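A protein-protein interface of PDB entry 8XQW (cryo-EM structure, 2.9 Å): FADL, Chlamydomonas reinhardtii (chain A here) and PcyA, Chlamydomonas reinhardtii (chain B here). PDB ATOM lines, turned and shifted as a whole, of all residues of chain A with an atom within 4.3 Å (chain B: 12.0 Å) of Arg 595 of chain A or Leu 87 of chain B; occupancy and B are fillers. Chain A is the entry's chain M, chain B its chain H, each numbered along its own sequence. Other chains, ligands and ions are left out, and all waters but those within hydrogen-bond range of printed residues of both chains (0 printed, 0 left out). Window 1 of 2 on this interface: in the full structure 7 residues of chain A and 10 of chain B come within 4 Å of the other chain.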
ATOM      1  N   VAL A 591     -20.462   5.458  35.027  1.00  0.00           N
ATOM      2  CA  VAL A 591     -20.896   4.115  34.667  1.00  0.00           C
ATOM      3  C   VAL A 591     -21.974   4.180  33.600  1.00  0.00           C
ATOM      4  O   VAL A 591     -21.852   3.573  32.529  1.00  0.00           O
ATOM      5  CB  VAL A 591     -21.389   3.362  35.909  1.00  0.00           C
ATOM      6  CG1 VAL A 591     -22.128   2.118  35.494  1.00  0.00           C
ATOM      7  CG2 VAL A 591     -20.226   3.022  36.819  1.00  0.00           C
ATOM      8  N   LEU A 592     -23.032   4.948  33.858  1.00  0.00           N
ATOM      9  CA  LEU A 592     -24.162   4.967  32.940  1.00  0.00           C
ATOM     10  C   LEU A 592     -23.772   5.531  31.585  1.00  0.00           C
ATOM     11  O   LEU A 592     -24.228   5.027  30.553  1.00  0.00           O
ATOM     12  CB  LEU A 592     -25.310   5.766  33.542  1.00  0.00           C
ATOM     13  CG  LEU A 592     -25.986   5.062  34.714  1.00  0.00           C
ATOM     14  CD1 LEU A 592     -27.058   5.933  35.306  1.00  0.00           C
ATOM     15  CD2 LEU A 592     -26.567   3.745  34.264  1.00  0.00           C
ATOM     16  N   ALA A 593     -22.919   6.553  31.566  1.00  0.00           N
ATOM     17  CA  ALA A 593     -22.457   7.112  30.305  1.00  0.00           C
ATOM     18  C   ALA A 593     -21.799   6.066  29.424  1.00  0.00           C
ATOM     19  O   ALA A 593     -21.770   6.230  28.201  1.00  0.00           O
ATOM     20  CB  ALA A 593     -21.483   8.258  30.561  1.00  0.00           C
ATOM     21  N   ALA A 594     -21.278   4.991  30.008  1.00  0.00           N
ATOM     22  CA  ALA A 594     -20.691   3.951  29.179  1.00  0.00           C
ATOM     23  C   ALA A 594     -21.767   3.128  28.487  1.00  0.00           C
ATOM     24  O   ALA A 594     -21.624   2.780  27.312  1.00  0.00           O
ATOM     25  CB  ALA A 594     -19.785   3.056  30.020  1.00  0.00           C
ATOM     26  N   ARG A 595     -22.857   2.823  29.187  1.00  0.00           N
ATOM     27  CA  ARG A 595     -23.843   1.890  28.659  1.00  0.00           C
ATOM     28  C   ARG A 595     -24.989   2.606  27.952  1.00  0.00           C
ATOM     29  O   ARG A 595     -25.446   2.161  26.895  1.00  0.00           O
ATOM     30  CB  ARG A 595     -24.368   1.003  29.788  1.00  0.00           C
ATOM     31  CG  ARG A 595     -23.273   0.447  30.657  1.00  0.00           C
ATOM     32  CD  ARG A 595     -22.493  -0.610  29.907  1.00  0.00           C
ATOM     33  NE  ARG A 595     -23.052  -1.943  30.097  1.00  0.00           N
ATOM     34  CZ  ARG A 595     -22.958  -2.638  31.226  1.00  0.00           C
ATOM     35  NH1 ARG A 595     -22.320  -2.133  32.272  1.00  0.00           N
ATOM     36  NH2 ARG A 595     -23.499  -3.844  31.306  1.00  0.00           N
ATOM     37  N   LEU A 596     -25.467   3.705  28.521  1.00  0.00           N
ATOM     38  CA  LEU A 596     -26.518   4.497  27.904  1.00  0.00           C
ATOM     39  C   LEU A 596     -25.970   5.605  27.014  1.00  0.00           C
ATOM     40  O   LEU A 596     -26.714   6.524  26.659  1.00  0.00           O
ATOM     41  CB  LEU A 596     -27.428   5.097  28.976  1.00  0.00           C
ATOM     42  CG  LEU A 596     -28.510   4.212  29.592  1.00  0.00           C
ATOM     43  CD1 LEU A 596     -29.285   3.513  28.494  1.00  0.00           C
ATOM     44  CD2 LEU A 596     -27.933   3.224  30.581  1.00  0.00           C
ATOM     45  N   GLY A 597     -24.696   5.528  26.643  1.00  0.00           N
ATOM     46  CA  GLY A 597     -24.006   6.584  25.940  1.00  0.00           C
ATOM     47  C   GLY A 597     -24.771   7.249  24.815  1.00  0.00           C
ATOM     48  O   GLY A 597     -25.072   8.443  24.873  1.00  0.00           O
ATOM     49  N   TYR A 599     -27.646   7.665  23.926  1.00  0.00           N
ATOM     50  CA  TYR A 599     -28.955   8.260  24.146  1.00  0.00           C
ATOM     51  C   TYR A 599     -28.922   9.513  25.005  1.00  0.00           C
ATOM     52  O   TYR A 599     -29.858  10.316  24.931  1.00  0.00           O
ATOM     53  CB  TYR A 599     -29.890   7.244  24.805  1.00  0.00           C
ATOM     54  CG  TYR A 599     -29.784   5.852  24.242  1.00  0.00           C
ATOM     55  CD1 TYR A 599     -30.546   5.466  23.154  1.00  0.00           C
ATOM     56  CD2 TYR A 599     -28.932   4.920  24.805  1.00  0.00           C
ATOM     57  CE1 TYR A 599     -30.456   4.197  22.640  1.00  0.00           C
ATOM     58  CE2 TYR A 599     -28.833   3.650  24.294  1.00  0.00           C
ATOM     59  CZ  TYR A 599     -29.597   3.294  23.214  1.00  0.00           C
ATOM     60  OH  TYR A 599     -29.499   2.024  22.704  1.00  0.00           O
ATOM     61  N   SER B  85     -19.473  -2.554  24.292  1.00  0.00           N
ATOM     62  CA  SER B  85     -19.811  -2.037  25.616  1.00  0.00           C
ATOM     63  C   SER B  85     -21.140  -1.259  25.663  1.00  0.00           C
ATOM     64  O   SER B  85     -21.945  -1.498  26.561  1.00  0.00           O
ATOM     65  CB  SER B  85     -18.669  -1.164  26.151  1.00  0.00           C
ATOM     66  OG  SER B  85     -18.999  -0.629  27.420  1.00  0.00           O
ATOM     67  N   PRO B  86     -21.388  -0.340  24.729  1.00  0.00           N
ATOM     68  CA  PRO B  86     -22.674   0.363  24.716  1.00  0.00           C
ATOM     69  C   PRO B  86     -23.797  -0.602  24.360  1.00  0.00           C
ATOM     70  O   PRO B  86     -23.575  -1.684  23.828  1.00  0.00           O
ATOM     71  CB  PRO B  86     -22.484   1.432  23.641  1.00  0.00           C
ATOM     72  CG  PRO B  86     -21.457   0.884  22.753  1.00  0.00           C
ATOM     73  CD  PRO B  86     -20.515   0.148  23.645  1.00  0.00           C
ATOM     74  N   LEU B  87     -25.020  -0.189  24.658  1.00  0.00           N
ATOM     75  CA  LEU B  87     -26.179  -1.047  24.493  1.00  0.00           C
ATOM     76  C   LEU B  87     -26.877  -0.743  23.175  1.00  0.00           C
ATOM     77  O   LEU B  87     -26.582   0.243  22.498  1.00  0.00           O
ATOM     78  CB  LEU B  87     -27.150  -0.892  25.667  1.00  0.00           C
ATOM     79  CG  LEU B  87     -27.047  -1.995  26.724  1.00  0.00           C
ATOM     80  CD1 LEU B  87     -25.601  -2.230  27.113  1.00  0.00           C
ATOM     81  CD2 LEU B  87     -27.883  -1.682  27.954  1.00  0.00           C
ATOM     82  N   SER B  88     -27.810  -1.611  22.824  1.00  0.00           N
ATOM     83  CA  SER B  88     -28.477  -1.613  21.534  1.00  0.00           C
ATOM     84  C   SER B  88     -29.917  -1.173  21.704  1.00  0.00           C
ATOM     85  O   SER B  88     -30.480  -1.268  22.799  1.00  0.00           O
ATOM     86  CB  SER B  88     -28.425  -3.013  20.903  1.00  0.00           C
ATOM     87  OG  SER B  88     -28.485  -4.018  21.894  1.00  0.00           O
ATOM     88  N   PRO B  89     -30.550  -0.683  20.636  1.00  0.00           N
ATOM     89  CA  PRO B  89     -31.965  -0.306  20.736  1.00  0.00           C
ATOM     90  C   PRO B  89     -32.885  -1.487  20.943  1.00  0.00           C
ATOM     91  O   PRO B  89     -34.100  -1.287  21.047  1.00  0.00           O
ATOM     92  CB  PRO B  89     -32.251   0.378  19.392  1.00  0.00           C
ATOM     93  CG  PRO B  89     -30.917   0.643  18.788  1.00  0.00           C
ATOM     94  CD  PRO B  89     -30.008  -0.417  19.296  1.00  0.00           C
ATOM     95  N   GLU B  90     -32.356  -2.708  20.995  1.00  0.00           N
ATOM     96  CA  GLU B  90     -33.205  -3.881  21.136  1.00  0.00           C
ATOM     97  C   GLU B  90     -33.019  -4.579  22.473  1.00  0.00           C
ATOM     98  O   GLU B  90     -34.009  -4.926  23.124  1.00  0.00           O
ATOM     99  CB  GLU B  90     -32.942  -4.865  19.995  1.00  0.00           C
ATOM    100  CG  GLU B  90     -31.480  -5.114  19.722  1.00  0.00           C
ATOM    101  CD  GLU B  90     -30.931  -6.250  20.550  1.00  0.00           C
ATOM    102  OE1 GLU B  90     -31.664  -7.237  20.760  1.00  0.00           O
ATOM    103  OE2 GLU B  90     -29.777  -6.148  21.014  1.00  0.00           O
ATOM    104  N   ASP B  91     -31.777  -4.778  22.911  1.00  0.00           N
ATOM    105  CA  ASP B  91     -31.545  -5.557  24.118  1.00  0.00           C
ATOM    106  C   ASP B  91     -32.088  -4.876  25.362  1.00  0.00           C
ATOM    107  O   ASP B  91     -32.183  -5.519  26.413  1.00  0.00           O
ATOM    108  CB  ASP B  91     -30.058  -5.852  24.289  1.00  0.00           C
ATOM    109  CG  ASP B  91     -29.301  -4.688  24.845  1.00  0.00           C
ATOM    110  OD1 ASP B  91     -29.219  -3.651  24.158  1.00  0.00           O
ATOM    111  OD2 ASP B  91     -28.791  -4.814  25.977  1.00  0.00           O
ATOM    112  N   ILE B  92     -32.458  -3.600  25.265  1.00  0.00           N
ATOM    113  CA  ILE B  92     -33.268  -2.987  26.308  1.00  0.00           C
ATOM    114  C   ILE B  92     -34.556  -3.778  26.494  1.00  0.00           C
ATOM    115  O   ILE B  92     -34.967  -4.076  27.624  1.00  0.00           O
ATOM    116  CB  ILE B  92     -33.550  -1.516  25.960  1.00  0.00           C
ATOM    117  CG1 ILE B  92     -32.242  -0.753  25.770  1.00  0.00           C
ATOM    118  CG2 ILE B  92     -34.373  -0.860  27.040  1.00  0.00           C
ATOM    119  CD1 ILE B  92     -31.281  -0.922  26.909  1.00  0.00           C
ATOM    120  N   MET B  93     -35.204  -4.145  25.388  1.00  0.00           N
ATOM    121  CA  MET B  93     -36.419  -4.941  25.485  1.00  0.00           C
ATOM    122  C   MET B  93     -36.127  -6.319  26.061  1.00  0.00           C
ATOM    123  O   MET B  93     -36.948  -6.878  26.796  1.00  0.00           O
ATOM    124  CB  MET B  93     -37.082  -5.058  24.118  1.00  0.00           C
ATOM    125  CG  MET B  93     -37.680  -3.759  23.635  1.00  0.00           C
ATOM    126  SD  MET B  93     -36.472  -2.768  22.747  1.00  0.00           S
ATOM    127  CE  MET B  93     -36.820  -3.245  21.058  1.00  0.00           C
ATOM    128  N   ARG B  94     -34.967  -6.884  25.735  1.00  0.00           N
ATOM    129  CA  ARG B  94     -34.566  -8.139  26.354  1.00  0.00           C
ATOM    130  C   ARG B  94     -34.482  -7.990  27.864  1.00  0.00           C
ATOM    131  O   ARG B  94     -34.918  -8.870  28.616  1.00  0.00           O
ATOM    132  CB  ARG B  94     -33.229  -8.591  25.779  1.00  0.00           C
ATOM    133  CG  ARG B  94     -32.812  -9.980  26.199  1.00  0.00           C
ATOM    134  CD  ARG B  94     -31.365 -10.249  25.832  1.00  0.00           C
ATOM    135  NE  ARG B  94     -30.878  -9.320  24.815  1.00  0.00           N
ATOM    136  CZ  ARG B  94     -31.002  -9.510  23.504  1.00  0.00           C
ATOM    137  NH1 ARG B  94     -31.611 -10.594  23.045  1.00  0.00           N
ATOM    138  NH2 ARG B  94     -30.525  -8.614  22.652  1.00  0.00           N
ATOM    139  N   LEU B  95     -33.927  -6.870  28.325  1.00  0.00           N
ATOM    140  CA  LEU B  95     -33.841  -6.622  29.759  1.00  0.00           C
ATOM    141  C   LEU B  95     -35.225  -6.509  30.381  1.00  0.00           C
ATOM    142  O   LEU B  95     -35.477  -7.057  31.460  1.00  0.00           O
ATOM    143  CB  LEU B  95     -33.034  -5.357  30.020  1.00  0.00           C
ATOM    144  CG  LEU B  95     -31.522  -5.539  30.070  1.00  0.00           C
ATOM    145  CD1 LEU B  95     -30.859  -4.260  30.523  1.00  0.00           C
ATOM    146  CD2 LEU B  95     -31.168  -6.683  30.990  1.00  0.00           C
ATOM    147  N   VAL B  96     -36.134  -5.808  29.706  1.00  0.00           N
ATOM    148  CA  VAL B  96     -37.497  -5.677  30.217  1.00  0.00           C
ATOM    149  C   VAL B  96     -38.146  -7.046  30.352  1.00  0.00           C
ATOM    150  O   VAL B  96     -38.763  -7.365  31.381  1.00  0.00           O
ATOM    151  CB  VAL B  96     -38.324  -4.768  29.293  1.00  0.00           C
ATOM    152  CG1 VAL B  96     -39.779  -4.806  29.690  1.00  0.00           C
ATOM    153  CG2 VAL B  96     -37.806  -3.358  29.330  1.00  0.00           C
ATOM    154  N   GLN B  97     -38.011  -7.874  29.317  1.00  0.00           N
ATOM    155  CA  GLN B  97     -38.610  -9.200  29.342  1.00  0.00           C
ATOM    156  C   GLN B  97     -38.055 -10.018  30.492  1.00  0.00           C
ATOM    157  O   GLN B  97     -38.810 -10.614  31.269  1.00  0.00           O
ATOM    158  CB  GLN B  97     -38.363  -9.911  28.017  1.00  0.00           C
ATOM    159  CG  GLN B  97     -39.165  -9.347  26.873  1.00  0.00           C
ATOM    160  CD  GLN B  97     -40.648  -9.531  27.072  1.00  0.00           C
ATOM    161  OE1 GLN B  97     -41.084 -10.464  27.743  1.00  0.00           O
ATOM    162  NE2 GLN B  97     -41.435  -8.637  26.493  1.00  0.00           N
ATOM    163  N   GLN B  98     -36.732 -10.064  30.611  1.00  0.00           N
ATOM    164  CA  GLN B  98     -36.120 -10.867  31.657  1.00  0.00           C
ATOM    165  C   GLN B  98     -36.559 -10.401  33.036  1.00  0.00           C
ATOM    166  O   GLN B  98     -36.820 -11.221  33.926  1.00  0.00           O
ATOM    167  CB  GLN B  98     -34.604 -10.815  31.518  1.00  0.00           C
ATOM    168  CG  GLN B  98     -33.854 -10.958  32.811  1.00  0.00           C
ATOM    169  CD  GLN B  98     -32.362 -10.963  32.595  1.00  0.00           C
ATOM    170  OE1 GLN B  98     -31.601 -10.439  33.408  1.00  0.00           O
ATOM    171  NE2 GLN B  98     -31.931 -11.554  31.489  1.00  0.00           N
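O of Arg 595 of chain A is in hydrogen-bond range of N of Leu 87 of chain B. The side-chain hydroxyl (OH) of Tyr 599 of chain A lies within hydrogen-bond range of the backbone carbonyl oxygen (O) of Leu 87 of chain B, at 3.4 Å. OH of Tyr 599 of chain A sits close to O of Ser 88 of chain B (3.4 Å).
OG of Ser 88 of chain B lies within hydrogen-bond range of OD1 of Asp 91 of chain B (2.4 Å). OG of Ser 88 of chain B lies within hydrogen-bond range of OE2 of Glu 90 of chain B (2.6 Å).
Among the printed residues, pairs that only touch across the chains: Ala 594 of chain A with Pro 86 of chain B (3.7 Å), Arg 595 of chain A with Ser 85 of chain B (3.5 Å), Arg 595 of chain A with Pro 86 of chain B (3.96 Å) and Tyr 599 of chain A with Pro 89 of chain B (3.6 Å).
Val 591 of chain A touches none of the printed residues of chain B. No residue of chain B comes within 4 Å of Leu 592 of chain A. No residue of chain B comes within 4 Å of Ala 593 of chain A. Of chain B, only Ser 85 (3.5 Å), Pro 86 (3.96 Å) and Leu 87 (3.3 Å) come within 4 Å of Arg 595 of chain A. No residue of chain B comes within 4 Å of Leu 596 of chain A. No residue of chain B comes within 4 Å of Gly 597 of chain A. Of the printed residues of chain B, Tyr 599 of chain A touches Leu 87, Ser 88 and Pro 89. Of the printed residues of chain A, Pro 86 of chain B touches Ala 594 (3.7 Å) and Arg 595 (3.96 Å). Printed residues of chain A within 4 Å of Leu 87 of chain B: Arg 595 (3.3 Å) and Tyr 599 (3.4 Å). The nearest printed residue of chain A that does not touch Leu 87 of chain B is Ala 594 of chain A (5.2 Å).
Of the 14 printed residues of chain B, 5 touch a printed residue of chain A. Printed residues of chain B that touch a printed residue of chain A: Ser 85, Pro 86, Leu 87, Ser 88 and Pro 89. Hydrophobic or aromatic side chains of chain B that line the printed part of chain A: Leu 87. Hydrophobic or aromatic side chains of chain A within 4 Å of the printed part of chain B: Tyr 599.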
